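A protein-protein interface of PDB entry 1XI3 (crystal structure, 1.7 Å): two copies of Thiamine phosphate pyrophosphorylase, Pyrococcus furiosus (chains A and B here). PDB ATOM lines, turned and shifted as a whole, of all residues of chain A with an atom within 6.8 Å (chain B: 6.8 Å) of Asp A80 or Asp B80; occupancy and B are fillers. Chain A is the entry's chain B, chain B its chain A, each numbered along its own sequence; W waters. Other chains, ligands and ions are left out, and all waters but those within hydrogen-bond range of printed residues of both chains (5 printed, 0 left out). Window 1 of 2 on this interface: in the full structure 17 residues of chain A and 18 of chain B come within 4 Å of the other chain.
Thr A52 touches Asp B77, and with the chains exchanged Asp A77 touches Thr B52. Arg B78 touches its own counterpart, Arg A78. Asp B80 touches its own counterpart, Asp A80. Asp A80 touches Ile B105, and with the chains exchanged Ile A105 touches Asp B80. Of the 20 pairs that touch across the chains among the printed residues, 20 have their exchanged pair printed and touching as well.
Among the printed residues, pairs that only touch across the chains: Thr A52 with Met B97 (3.9 Å), Tyr A56 with Val B101 (3.4 Å), Asp A80 with Asp B80 (3.5 Å), Asp A80 with Met B97 (3.6 Å), Asp A80 with Ile B105 (3.8 Å), Leu A83 with Ile B105 (3.9 Å), Ala A84 with Met B97 (3.6 Å), Ala A84 with Val B101 (3.6 Å), Ala A84 with Ile B105 (3.9 Å), Met A97 with Thr B52 (3.8 Å), Met A97 with Asp B80 (3.6 Å), Met A97 with Ala B84 (3.8 Å), Val A101 with Tyr B56 (3.3 Å), Val A101 with Ala B84 (3.5 Å), Ile A105 with Asp B80 (3.8 Å), Ile A105 with Leu B83 (3.9 Å) and Ile A105 with Ala B84 (3.9 Å).
The guanidinium group (NH2) of Arg B78 lies within salt-bridge range of the side-chain carboxylate (OD2) of Asp B80 (2.8 Å). The side-chain sulfur of Met A55 lies within hydrogen-bond range of the guanidinium group of Arg A78 (3.5 Å). SD of Met B55 lies within hydrogen-bond range of NH1 of Arg B78. The side-chain hydroxyl (OG1) of Thr B52 sits at hydrogen-bond distance from the guanidinium group (NH2) of Arg B78, 2.9 Å away. NH2 of Arg A78 lies within hydrogen-bond range of OG1 of Thr A52 (2.9 Å). NH2 of Arg A78 lies within salt-bridge range of OD2 of Asp A80, 2.8 Å away.
Water W2 lies within hydrogen-bond range of the side-chain carboxylate of Asp B77 (2.6 Å) and the side-chain hydroxyl of Thr A52 (3.4 Å). Water W1 lies within hydrogen-bond range of the side-chain carboxylate (OD2) of Asp B80 (2.7 Å), the backbone NH (N) of Val A79 (2.9 Å) and the backbone carbonyl oxygen (O) of Asp A77 (3.2 Å). Water W5 lies within hydrogen-bond range of the side-chain carboxylate (OD2) of Asp A80 (2.7 Å), the backbone NH (N) of Val B79 (2.8 Å) and the backbone carbonyl oxygen (O) of Asp B77 (3.1 Å). Water W3 bridges OD2 of Asp A77 and N of Thr B52. Water W4 lies within hydrogen-bond range of OD1 of Asp B77 (2.8 Å) and N of Thr A52 (2.9 Å).
The guanidinium group (NE) of Arg A78 lies close to the guanidinium group (NE) of Arg B78 (3.3 Å). The side-chain carboxylate (OD2) of Asp B77 lies within hydrogen-bond range of the side-chain hydroxyl (OG1) of Thr A52. The side-chain hydroxyl (OG1) of Thr B52 is in hydrogen-bond range of the side-chain carboxylate (OD1) of Asp A77 (2.8 Å).
Of the 17 printed residues of chain A, 10 touch a printed residue of chain B. Hydrophobic or aromatic side chains of chain A that line the printed part of chain B: Tyr A56, Leu A83, Ala A84, Met A97, Val A101 and Ile A105. Printed residues of chain B that touch a printed residue of chain A: Thr B52, Tyr B56, Asp B77, Arg B78, Asp B80, Leu B83, Ala B84, Met B97, Val B101 and Ile B105. Hydrophobic or aromatic side chains of chain B that line the printed part of chain A: Tyr B56, Ala B84, Met B97, Val B101 and Ile B105. Among the printed residues, 20 pairs touch across the chains. Among the printed residues, no Asp or Glu carboxylate lies within 4 Å of a Lys or Arg side-chain nitrogen of the other chain.
Printed residues of chain B within 4 Å of Thr A52: Asp B77 and Met B97. Of the printed residues of chain B, Tyr A56 touches Val B101 (3.4 Å). Of the printed residues of chain B, Arg A78 touches Arg B78 (3.3 Å). Printed residues of chain B within 4 Å of Asp A80: Asp B80 (3.5 Å), Met B97 (3.6 Å) and Ile B105 (3.8 Å). Of the printed residues of chain A, Asp B80 touches Asp A80, Met A97 and Ile A105. Of the printed residues of chain A, Leu B83 touches Ile A105. The nearest printed residue of chain B that does not touch Asp A80 is Arg B78 (4.3 Å).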
ATOM      1  N   THR A  52      24.307  23.532 -39.334  1.00  0.00           N
ATOM      2  CA  THR A  52      25.439  22.908 -38.656  1.00  0.00           C
ATOM      3  C   THR A  52      26.208  21.900 -39.539  1.00  0.00           C
ATOM      4  O   THR A  52      27.441  21.847 -39.496  1.00  0.00           O
ATOM      5  CB  THR A  52      24.974  22.278 -37.321  1.00  0.00           C
ATOM      6  OG1 THR A  52      24.344  23.300 -36.536  1.00  0.00           O
ATOM      7  CG2 THR A  52      26.121  21.720 -36.565  1.00  0.00           C
ATOM      8  N   MET A  55      28.597  23.794 -41.742  1.00  0.00           N
ATOM      9  CA  MET A  55      29.723  24.325 -40.975  1.00  0.00           C
ATOM     10  C   MET A  55      30.733  23.222 -40.682  1.00  0.00           C
ATOM     11  O   MET A  55      31.974  23.428 -40.721  1.00  0.00           O
ATOM     12  CB  MET A  55      29.209  24.952 -39.661  1.00  0.00           C
ATOM     13  CG  MET A  55      28.356  26.143 -39.867  1.00  0.00           C
ATOM     14  SD  MET A  55      27.823  26.770 -38.247  1.00  0.00           S
ATOM     15  CE  MET A  55      26.885  28.222 -38.779  1.00  0.00           C
ATOM     16  N   TYR A  56      30.216  22.047 -40.340  1.00  0.00           N
ATOM     17  CA  TYR A  56      31.061  20.877 -40.058  1.00  0.00           C
ATOM     18  C   TYR A  56      31.886  20.469 -41.290  1.00  0.00           C
ATOM     19  O   TYR A  56      33.101  20.283 -41.201  1.00  0.00           O
ATOM     20  CB  TYR A  56      30.182  19.736 -39.584  1.00  0.00           C
ATOM     21  CG  TYR A  56      30.876  18.410 -39.517  1.00  0.00           C
ATOM     22  CD1 TYR A  56      30.634  17.429 -40.460  1.00  0.00           C
ATOM     23  CD2 TYR A  56      31.834  18.166 -38.549  1.00  0.00           C
ATOM     24  CE1 TYR A  56      31.298  16.236 -40.426  1.00  0.00           C
ATOM     25  CE2 TYR A  56      32.505  16.965 -38.513  1.00  0.00           C
ATOM     26  CZ  TYR A  56      32.220  16.008 -39.461  1.00  0.00           C
ATOM     27  OH  TYR A  56      32.918  14.791 -39.399  1.00  0.00           O
ATOM     28  N   ASP A  77      32.585  31.592 -32.470  1.00  0.00           N
ATOM     29  CA  ASP A  77      31.349  31.308 -31.718  1.00  0.00           C
ATOM     30  C   ASP A  77      31.213  29.816 -31.400  1.00  0.00           C
ATOM     31  O   ASP A  77      31.266  29.417 -30.230  1.00  0.00           O
ATOM     32  CB  ASP A  77      30.150  31.905 -32.483  1.00  0.00           C
ATOM     33  CG  ASP A  77      28.769  31.687 -31.838  1.00  0.00           C
ATOM     34  OD1 ASP A  77      28.582  30.991 -30.822  1.00  0.00           O
ATOM     35  OD2 ASP A  77      27.834  32.287 -32.449  1.00  0.00           O
ATOM     36  N   ARG A  78      31.137  28.978 -32.434  1.00  0.00           N
ATOM     37  CA  ARG A  78      30.542  27.654 -32.323  1.00  0.00           C
ATOM     38  C   ARG A  78      31.492  26.586 -31.753  1.00  0.00           C
ATOM     39  O   ARG A  78      32.321  25.969 -32.450  1.00  0.00           O
ATOM     40  CB  ARG A  78      29.975  27.238 -33.684  1.00  0.00           C
ATOM     41  CG  ARG A  78      28.830  28.094 -34.191  1.00  0.00           C
ATOM     42  CD  ARG A  78      27.544  27.835 -33.405  1.00  0.00           C
ATOM     43  NE  ARG A  78      27.127  26.461 -33.601  1.00  0.00           N
ATOM     44  CZ  ARG A  78      26.303  26.058 -34.569  1.00  0.00           C
ATOM     45  NH1 ARG A  78      25.738  26.928 -35.392  1.00  0.00           N
ATOM     46  NH2 ARG A  78      26.046  24.796 -34.693  1.00  0.00           N
ATOM     47  N   VAL A  79      31.356  26.339 -30.466  1.00  0.00           N
ATOM     48  CA  VAL A  79      32.190  25.343 -29.787  1.00  0.00           C
ATOM     49  C   VAL A  79      31.954  23.910 -30.272  1.00  0.00           C
ATOM     50  O   VAL A  79      32.888  23.091 -30.343  1.00  0.00           O
ATOM     51  CB  VAL A  79      31.989  25.432 -28.250  1.00  0.00           C
ATOM     52  CG1 VAL A  79      32.733  24.305 -27.491  1.00  0.00           C
ATOM     53  CG2 VAL A  79      32.444  26.757 -27.708  1.00  0.00           C
ATOM     54  N   ASP A  80      30.702  23.591 -30.594  1.00  0.00           N
ATOM     55  CA  ASP A  80      30.351  22.291 -31.175  1.00  0.00           C
ATOM     56  C   ASP A  80      31.145  22.053 -32.446  1.00  0.00           C
ATOM     57  O   ASP A  80      31.724  20.983 -32.664  1.00  0.00           O
ATOM     58  CB  ASP A  80      28.863  22.152 -31.444  1.00  0.00           C
ATOM     59  CG  ASP A  80      28.272  23.267 -32.293  1.00  0.00           C
ATOM     60  OD1 ASP A  80      28.702  24.425 -32.189  1.00  0.00           O
ATOM     61  OD2 ASP A  80      27.295  22.979 -33.048  1.00  0.00           O
ATOM     62  N   VAL A  81      31.161  23.064 -33.281  1.00  0.00           N
ATOM     63  CA  VAL A  81      31.820  22.928 -34.582  1.00  0.00           C
ATOM     64  C   VAL A  81      33.325  22.791 -34.373  1.00  0.00           C
ATOM     65  O   VAL A  81      33.945  21.905 -34.931  1.00  0.00           O
ATOM     66  CB  VAL A  81      31.452  24.092 -35.536  1.00  0.00           C
ATOM     67  CG1 VAL A  81      32.246  24.000 -36.835  1.00  0.00           C
ATOM     68  CG2 VAL A  81      29.938  24.068 -35.841  1.00  0.00           C
ATOM     69  N   ALA A  82      33.886  23.627 -33.516  1.00  0.00           N
ATOM     70  CA  ALA A  82      35.307  23.532 -33.185  1.00  0.00           C
ATOM     71  C   ALA A  82      35.659  22.151 -32.677  1.00  0.00           C
ATOM     72  O   ALA A  82      36.657  21.532 -33.130  1.00  0.00           O
ATOM     73  CB  ALA A  82      35.669  24.608 -32.190  1.00  0.00           C
ATOM     74  N   LEU A  83      34.862  21.625 -31.747  1.00  0.00           N
ATOM     75  CA  LEU A  83      35.126  20.282 -31.252  1.00  0.00           C
ATOM     76  C   LEU A  83      35.044  19.218 -32.358  1.00  0.00           C
ATOM     77  O   LEU A  83      35.946  18.350 -32.465  1.00  0.00           O
ATOM     78  CB  LEU A  83      34.184  19.912 -30.107  1.00  0.00           C
ATOM     79  CG  LEU A  83      34.332  20.671 -28.799  1.00  0.00           C
ATOM     80  CD1 LEU A  83      33.165  20.317 -27.840  1.00  0.00           C
ATOM     81  CD2 LEU A  83      35.653  20.324 -28.163  1.00  0.00           C
ATOM     82  N   ALA A  84      33.985  19.292 -33.159  1.00  0.00           N
ATOM     83  CA  ALA A  84      33.683  18.284 -34.180  1.00  0.00           C
ATOM     84  C   ALA A  84      34.804  18.211 -35.230  1.00  0.00           C
ATOM     85  O   ALA A  84      35.107  17.126 -35.766  1.00  0.00           O
ATOM     86  CB  ALA A  84      32.376  18.599 -34.831  1.00  0.00           C
ATOM     87  N   VAL A  85      35.408  19.354 -35.529  1.00  0.00           N
ATOM     88  CA  VAL A  85      36.442  19.424 -36.608  1.00  0.00           C
ATOM     89  C   VAL A  85      37.861  19.421 -36.100  1.00  0.00           C
ATOM     90  O   VAL A  85      38.794  19.573 -36.876  1.00  0.00           O
ATOM     91  CB  VAL A  85      36.178  20.610 -37.615  1.00  0.00           C
ATOM     92  CG1 VAL A  85      34.711  20.556 -38.105  1.00  0.00           C
ATOM     93  CG2 VAL A  85      36.556  21.934 -37.005  1.00  0.00           C
ATOM     94  N   VAL A  90      38.459  28.376 -30.341  1.00  0.00           N
ATOM     95  CA  VAL A  90      37.210  29.065 -30.601  1.00  0.00           C
ATOM     96  C   VAL A  90      37.387  30.504 -30.166  1.00  0.00           C
ATOM     97  O   VAL A  90      38.092  30.779 -29.183  1.00  0.00           O
ATOM     98  CB  VAL A  90      36.025  28.372 -29.857  1.00  0.00           C
ATOM     99  CG1 VAL A  90      36.225  28.454 -28.310  1.00  0.00           C
ATOM    100  CG2 VAL A  90      34.739  28.926 -30.277  1.00  0.00           C
ATOM    101  N   MET A  97      28.839  31.882 -26.048  1.00  0.00           N
ATOM    102  CA  MET A  97      28.984  31.119 -24.817  1.00  0.00           C
ATOM    103  C   MET A  97      29.931  31.814 -23.878  1.00  0.00           C
ATOM    104  O   MET A  97      30.972  32.250 -24.297  1.00  0.00           O
ATOM    105  CB  MET A  97      29.535  29.729 -25.126  1.00  0.00           C
ATOM    106  CG  MET A  97      29.386  28.777 -23.974  1.00  0.00           C
ATOM    107  SD  MET A  97      29.745  27.086 -24.365  1.00  0.00           S
ATOM    108  CE  MET A  97      28.326  26.678 -25.436  1.00  0.00           C
ATOM    109  N   VAL A 101      32.148  28.729 -19.266  1.00  0.00           N
ATOM    110  CA  VAL A 101      31.330  27.584 -19.700  1.00  0.00           C
ATOM    111  C   VAL A 101      32.000  26.857 -20.893  1.00  0.00           C
ATOM    112  O   VAL A 101      32.074  25.646 -20.902  1.00  0.00           O
ATOM    113  CB  VAL A 101      29.901  28.028 -20.087  1.00  0.00           C
ATOM    114  CG1 VAL A 101      29.048  26.842 -20.523  1.00  0.00           C
ATOM    115  CG2 VAL A 101      29.207  28.764 -18.916  1.00  0.00           C
ATOM    116  N   ILE A 105      33.160  22.803 -21.054  1.00  0.00           N
ATOM    117  CA  ILE A 105      32.733  21.786 -21.997  1.00  0.00           C
ATOM    118  C   ILE A 105      33.792  21.437 -23.044  1.00  0.00           C
ATOM    119  O   ILE A 105      33.690  20.394 -23.702  1.00  0.00           O
ATOM    120  CB  ILE A 105      31.390  22.168 -22.715  1.00  0.00           C
ATOM    121  CG1 ILE A 105      31.590  23.358 -23.632  1.00  0.00           C
ATOM    122  CG2 ILE A 105      30.311  22.465 -21.675  1.00  0.00           C
ATOM    123  CD1 ILE A 105      30.377  23.621 -24.550  1.00  0.00           C
ATOM    124  N   LEU A 109      40.347  23.235 -26.014  1.00  0.00           N
ATOM    125  CA  LEU A 109      40.337  24.308 -26.996  1.00  0.00           C
ATOM    126  C   LEU A 109      41.061  25.529 -26.491  1.00  0.00           C
ATOM    127  O   LEU A 109      41.004  25.874 -25.307  1.00  0.00           O
ATOM    128  CB  LEU A 109      38.898  24.712 -27.389  1.00  0.00           C
ATOM    129  CG  LEU A 109      38.109  23.670 -28.173  1.00  0.00           C
ATOM    130  CD1 LEU A 109      36.709  24.211 -28.488  1.00  0.00           C
ATOM    131  CD2 LEU A 109      38.836  23.239 -29.457  1.00  0.00           C
ATOM    132  N   THR B  52      24.130  32.528 -29.284  1.00  0.00           N
ATOM    133  CA  THR B  52      24.450  31.431 -28.417  1.00  0.00           C
ATOM    134  C   THR B  52      24.274  31.781 -26.946  1.00  0.00           C
ATOM    135  O   THR B  52      23.783  30.970 -26.160  1.00  0.00           O
ATOM    136  CB  THR B  52      25.865  30.956 -28.701  1.00  0.00           C
ATOM    137  OG1 THR B  52      25.955  30.584 -30.072  1.00  0.00           O
ATOM    138  CG2 THR B  52      26.215  29.787 -27.840  1.00  0.00           C
ATOM    139  N   MET B  55      20.569  31.373 -26.141  1.00  0.00           N
ATOM    140  CA  MET B  55      20.256  29.933 -26.084  1.00  0.00           C
ATOM    141  C   MET B  55      20.744  29.310 -24.759  1.00  0.00           C
ATOM    142  O   MET B  55      20.036  28.526 -24.123  1.00  0.00           O
ATOM    143  CB  MET B  55      20.882  29.215 -27.281  1.00  0.00           C
ATOM    144  CG  MET B  55      20.350  29.706 -28.618  1.00  0.00           C
ATOM    145  SD  MET B  55      21.112  28.711 -29.894  1.00  0.00           S
ATOM    146  CE  MET B  55      20.228  29.178 -31.349  1.00  0.00           C
ATOM    147  N   TYR B  56      21.939  29.712 -24.316  1.00  0.00           N
ATOM    148  CA  TYR B  56      22.515  29.225 -23.098  1.00  0.00           C
ATOM    149  C   TYR B  56      21.703  29.689 -21.899  1.00  0.00           C
ATOM    150  O   TYR B  56      21.367  28.884 -21.031  1.00  0.00           O
ATOM    151  CB  TYR B  56      23.960  29.705 -22.977  1.00  0.00           C
ATOM    152  CG  TYR B  56      24.551  29.505 -21.607  1.00  0.00           C
ATOM    153  CD1 TYR B  56      24.747  30.575 -20.751  1.00  0.00           C
ATOM    154  CD2 TYR B  56      24.880  28.256 -21.175  1.00  0.00           C
ATOM    155  CE1 TYR B  56      25.233  30.372 -19.475  1.00  0.00           C
ATOM    156  CE2 TYR B  56      25.396  28.044 -19.885  1.00  0.00           C
ATOM    157  CZ  TYR B  56      25.584  29.103 -19.083  1.00  0.00           C
ATOM    158  OH  TYR B  56      26.085  28.861 -17.822  1.00  0.00           O
ATOM    159  N   ASP B  77      19.316  20.344 -32.393  1.00  0.00           N
ATOM    160  CA  ASP B  77      20.521  20.677 -33.203  1.00  0.00           C
ATOM    161  C   ASP B  77      21.761  20.870 -32.349  1.00  0.00           C
ATOM    162  O   ASP B  77      22.733  20.107 -32.458  1.00  0.00           O
ATOM    163  CB  ASP B  77      20.172  21.944 -34.031  1.00  0.00           C
ATOM    164  CG  ASP B  77      21.253  22.424 -34.998  1.00  0.00           C
ATOM    165  OD1 ASP B  77      20.896  23.352 -35.801  1.00  0.00           O
ATOM    166  OD2 ASP B  77      22.405  21.984 -34.979  1.00  0.00           O
ATOM    167  N   ARG B  78      21.722  21.876 -31.490  1.00  0.00           N
ATOM    168  CA  ARG B  78      22.935  22.477 -30.923  1.00  0.00           C
ATOM    169  C   ARG B  78      23.554  21.674 -29.783  1.00  0.00           C
ATOM    170  O   ARG B  78      23.141  21.794 -28.617  1.00  0.00           O
ATOM    171  CB  ARG B  78      22.650  23.966 -30.493  1.00  0.00           C
ATOM    172  CG  ARG B  78      22.280  24.868 -31.653  1.00  0.00           C
ATOM    173  CD  ARG B  78      23.539  25.168 -32.488  1.00  0.00           C
ATOM    174  NE  ARG B  78      24.476  25.940 -31.703  1.00  0.00           N
ATOM    175  CZ  ARG B  78      24.447  27.271 -31.608  1.00  0.00           C
ATOM    176  NH1 ARG B  78      23.578  27.975 -32.278  1.00  0.00           N
ATOM    177  NH2 ARG B  78      25.294  27.879 -30.827  1.00  0.00           N
ATOM    178  N   VAL B  79      24.587  20.884 -30.119  1.00  0.00           N
ATOM    179  CA  VAL B  79      25.306  20.057 -29.138  1.00  0.00           C
ATOM    180  C   VAL B  79      26.074  20.947 -28.115  1.00  0.00           C
ATOM    181  O   VAL B  79      26.197  20.608 -26.930  1.00  0.00           O
ATOM    182  CB  VAL B  79      26.250  19.117 -29.855  1.00  0.00           C
ATOM    183  CG1 VAL B  79      27.143  18.382 -28.871  1.00  0.00           C
ATOM    184  CG2 VAL B  79      25.496  18.161 -30.748  1.00  0.00           C
ATOM    185  N   ASP B  80      26.577  22.088 -28.570  1.00  0.00           N
ATOM    186  CA  ASP B  80      27.280  23.035 -27.680  1.00  0.00           C
ATOM    187  C   ASP B  80      26.348  23.493 -26.579  1.00  0.00           C
ATOM    188  O   ASP B  80      26.702  23.483 -25.384  1.00  0.00           O
ATOM    189  CB  ASP B  80      27.864  24.247 -28.416  1.00  0.00           C
ATOM    190  CG  ASP B  80      26.859  24.995 -29.289  1.00  0.00           C
ATOM    191  OD1 ASP B  80      25.946  24.361 -29.846  1.00  0.00           O
ATOM    192  OD2 ASP B  80      27.037  26.243 -29.437  1.00  0.00           O
ATOM    193  N   VAL B  81      25.154  23.899 -26.982  1.00  0.00           N
ATOM    194  CA  VAL B  81      24.160  24.365 -26.013  1.00  0.00           C
ATOM    195  C   VAL B  81      23.748  23.234 -25.058  1.00  0.00           C
ATOM    196  O   VAL B  81      23.715  23.426 -23.856  1.00  0.00           O
ATOM    197  CB  VAL B  81      22.976  24.985 -26.712  1.00  0.00           C
ATOM    198  CG1 VAL B  81      21.875  25.370 -25.694  1.00  0.00           C
ATOM    199  CG2 VAL B  81      23.430  26.233 -27.510  1.00  0.00           C
ATOM    200  N   ALA B  82      23.470  22.059 -25.619  1.00  0.00           N
ATOM    201  CA  ALA B  82      23.108  20.888 -24.834  1.00  0.00           C
ATOM    202  C   ALA B  82      24.183  20.611 -23.787  1.00  0.00           C
ATOM    203  O   ALA B  82      23.884  20.384 -22.631  1.00  0.00           O
ATOM    204  CB  ALA B  82      22.886  19.682 -25.734  1.00  0.00           C
ATOM    205  N   LEU B  83      25.440  20.643 -24.202  1.00  0.00           N
ATOM    206  CA  LEU B  83      26.520  20.360 -23.232  1.00  0.00           C
ATOM    207  C   LEU B  83      26.584  21.459 -22.158  1.00  0.00           C
ATOM    208  O   LEU B  83      26.716  21.161 -20.949  1.00  0.00           O
ATOM    209  CB  LEU B  83      27.854  20.252 -23.948  1.00  0.00           C
ATOM    210  CG  LEU B  83      28.053  19.001 -24.809  1.00  0.00           C
ATOM    211  CD1 LEU B  83      29.329  19.171 -25.608  1.00  0.00           C
ATOM    212  CD2 LEU B  83      28.148  17.748 -23.974  1.00  0.00           C
ATOM    213  N   ALA B  84      26.516  22.708 -22.595  1.00  0.00           N
ATOM    214  CA  ALA B  84      26.712  23.864 -21.698  1.00  0.00           C
ATOM    215  C   ALA B  84      25.617  23.917 -20.626  1.00  0.00           C
ATOM    216  O   ALA B  84      25.895  24.301 -19.491  1.00  0.00           O
ATOM    217  CB  ALA B  84      26.712  25.109 -22.435  1.00  0.00           C
ATOM    218  N   VAL B  85      24.393  23.529 -20.977  1.00  0.00           N
ATOM    219  CA  VAL B  85      23.266  23.551 -20.001  1.00  0.00           C
ATOM    220  C   VAL B  85      22.980  22.190 -19.337  1.00  0.00           C
ATOM    221  O   VAL B  85      22.031  22.066 -18.534  1.00  0.00           O
ATOM    222  CB  VAL B  85      21.997  24.162 -20.616  1.00  0.00           C
ATOM    223  CG1 VAL B  85      22.316  25.486 -21.279  1.00  0.00           C
ATOM    224  CG2 VAL B  85      21.292  23.183 -21.543  1.00  0.00           C
ATOM    225  N   VAL B  90      20.231  15.698 -27.234  1.00  0.00           N
ATOM    226  CA  VAL B  90      20.136  16.590 -28.392  1.00  0.00           C
ATOM    227  C   VAL B  90      19.342  15.845 -29.481  1.00  0.00           C
ATOM    228  O   VAL B  90      19.436  14.621 -29.597  1.00  0.00           O
ATOM    229  CB  VAL B  90      21.539  16.979 -28.921  1.00  0.00           C
ATOM    230  CG1 VAL B  90      22.333  15.727 -29.337  1.00  0.00           C
ATOM    231  CG2 VAL B  90      21.449  18.011 -30.023  1.00  0.00           C
ATOM    232  N   MET B  97      24.696  18.163 -37.045  1.00  0.00           N
ATOM    233  CA  MET B  97      25.873  17.331 -36.878  1.00  0.00           C
ATOM    234  C   MET B  97      25.563  15.872 -37.092  1.00  0.00           C
ATOM    235  O   MET B  97      24.562  15.386 -36.619  1.00  0.00           O
ATOM    236  CB  MET B  97      26.416  17.495 -35.452  1.00  0.00           C
ATOM    237  CG  MET B  97      27.790  16.941 -35.306  1.00  0.00           C
ATOM    238  SD  MET B  97      28.543  17.459 -33.779  1.00  0.00           S
ATOM    239  CE  MET B  97      28.915  19.202 -34.138  1.00  0.00           C
ATOM    240  N   VAL B 101      29.434  11.844 -35.088  1.00  0.00           N
ATOM    241  CA  VAL B 101      30.295  12.922 -34.673  1.00  0.00           C
ATOM    242  C   VAL B 101      29.788  13.490 -33.364  1.00  0.00           C
ATOM    243  O   VAL B 101      30.567  13.798 -32.456  1.00  0.00           O
ATOM    244  CB  VAL B 101      30.342  14.032 -35.796  1.00  0.00           C
ATOM    245  CG1 VAL B 101      31.147  15.241 -35.334  1.00  0.00           C
ATOM    246  CG2 VAL B 101      30.922  13.449 -37.059  1.00  0.00           C
ATOM    247  N   ILE B 105      31.869  13.792 -29.664  1.00  0.00           N
ATOM    248  CA  ILE B 105      32.142  14.997 -28.909  1.00  0.00           C
ATOM    249  C   ILE B 105      31.296  15.133 -27.634  1.00  0.00           C
ATOM    250  O   ILE B 105      31.654  15.897 -26.733  1.00  0.00           O
ATOM    251  CB  ILE B 105      32.034  16.286 -29.775  1.00  0.00           C
ATOM    252  CG1 ILE B 105      30.622  16.524 -30.307  1.00  0.00           C
ATOM    253  CG2 ILE B 105      32.989  16.193 -30.936  1.00  0.00           C
ATOM    254  CD1 ILE B 105      30.432  17.919 -30.821  1.00  0.00           C
ATOM    255  N   LEU B 109      25.400  12.403 -23.949  1.00  0.00           N
ATOM    256  CA  LEU B 109      24.102  12.870 -24.376  1.00  0.00           C
ATOM    257  C   LEU B 109      23.275  11.766 -25.006  1.00  0.00           C
ATOM    258  O   LEU B 109      23.797  10.915 -25.755  1.00  0.00           O
ATOM    259  CB  LEU B 109      24.241  14.037 -25.408  1.00  0.00           C
ATOM    260  CG  LEU B 109      24.757  15.346 -24.908  1.00  0.00           C
ATOM    261  CD1 LEU B 109      24.821  16.331 -26.069  1.00  0.00           C
ATOM    262  CD2 LEU B 109      23.974  15.928 -23.747  1.00  0.00           C
HETATM  263  O   HOH W   1      29.336  27.408 -28.704  1.00  0.00           O
HETATM  264  O   HOH W   2      21.912  25.724 -36.368  1.00  0.00           O
HETATM  265  O   HOH W   3      26.189  33.801 -30.923  1.00  0.00           O
HETATM  266  O   HOH W   4      21.610  22.981 -38.473  1.00  0.00           O
HETATM  267  O   HOH W   5      25.756  20.785 -32.697  1.00  0.00           O
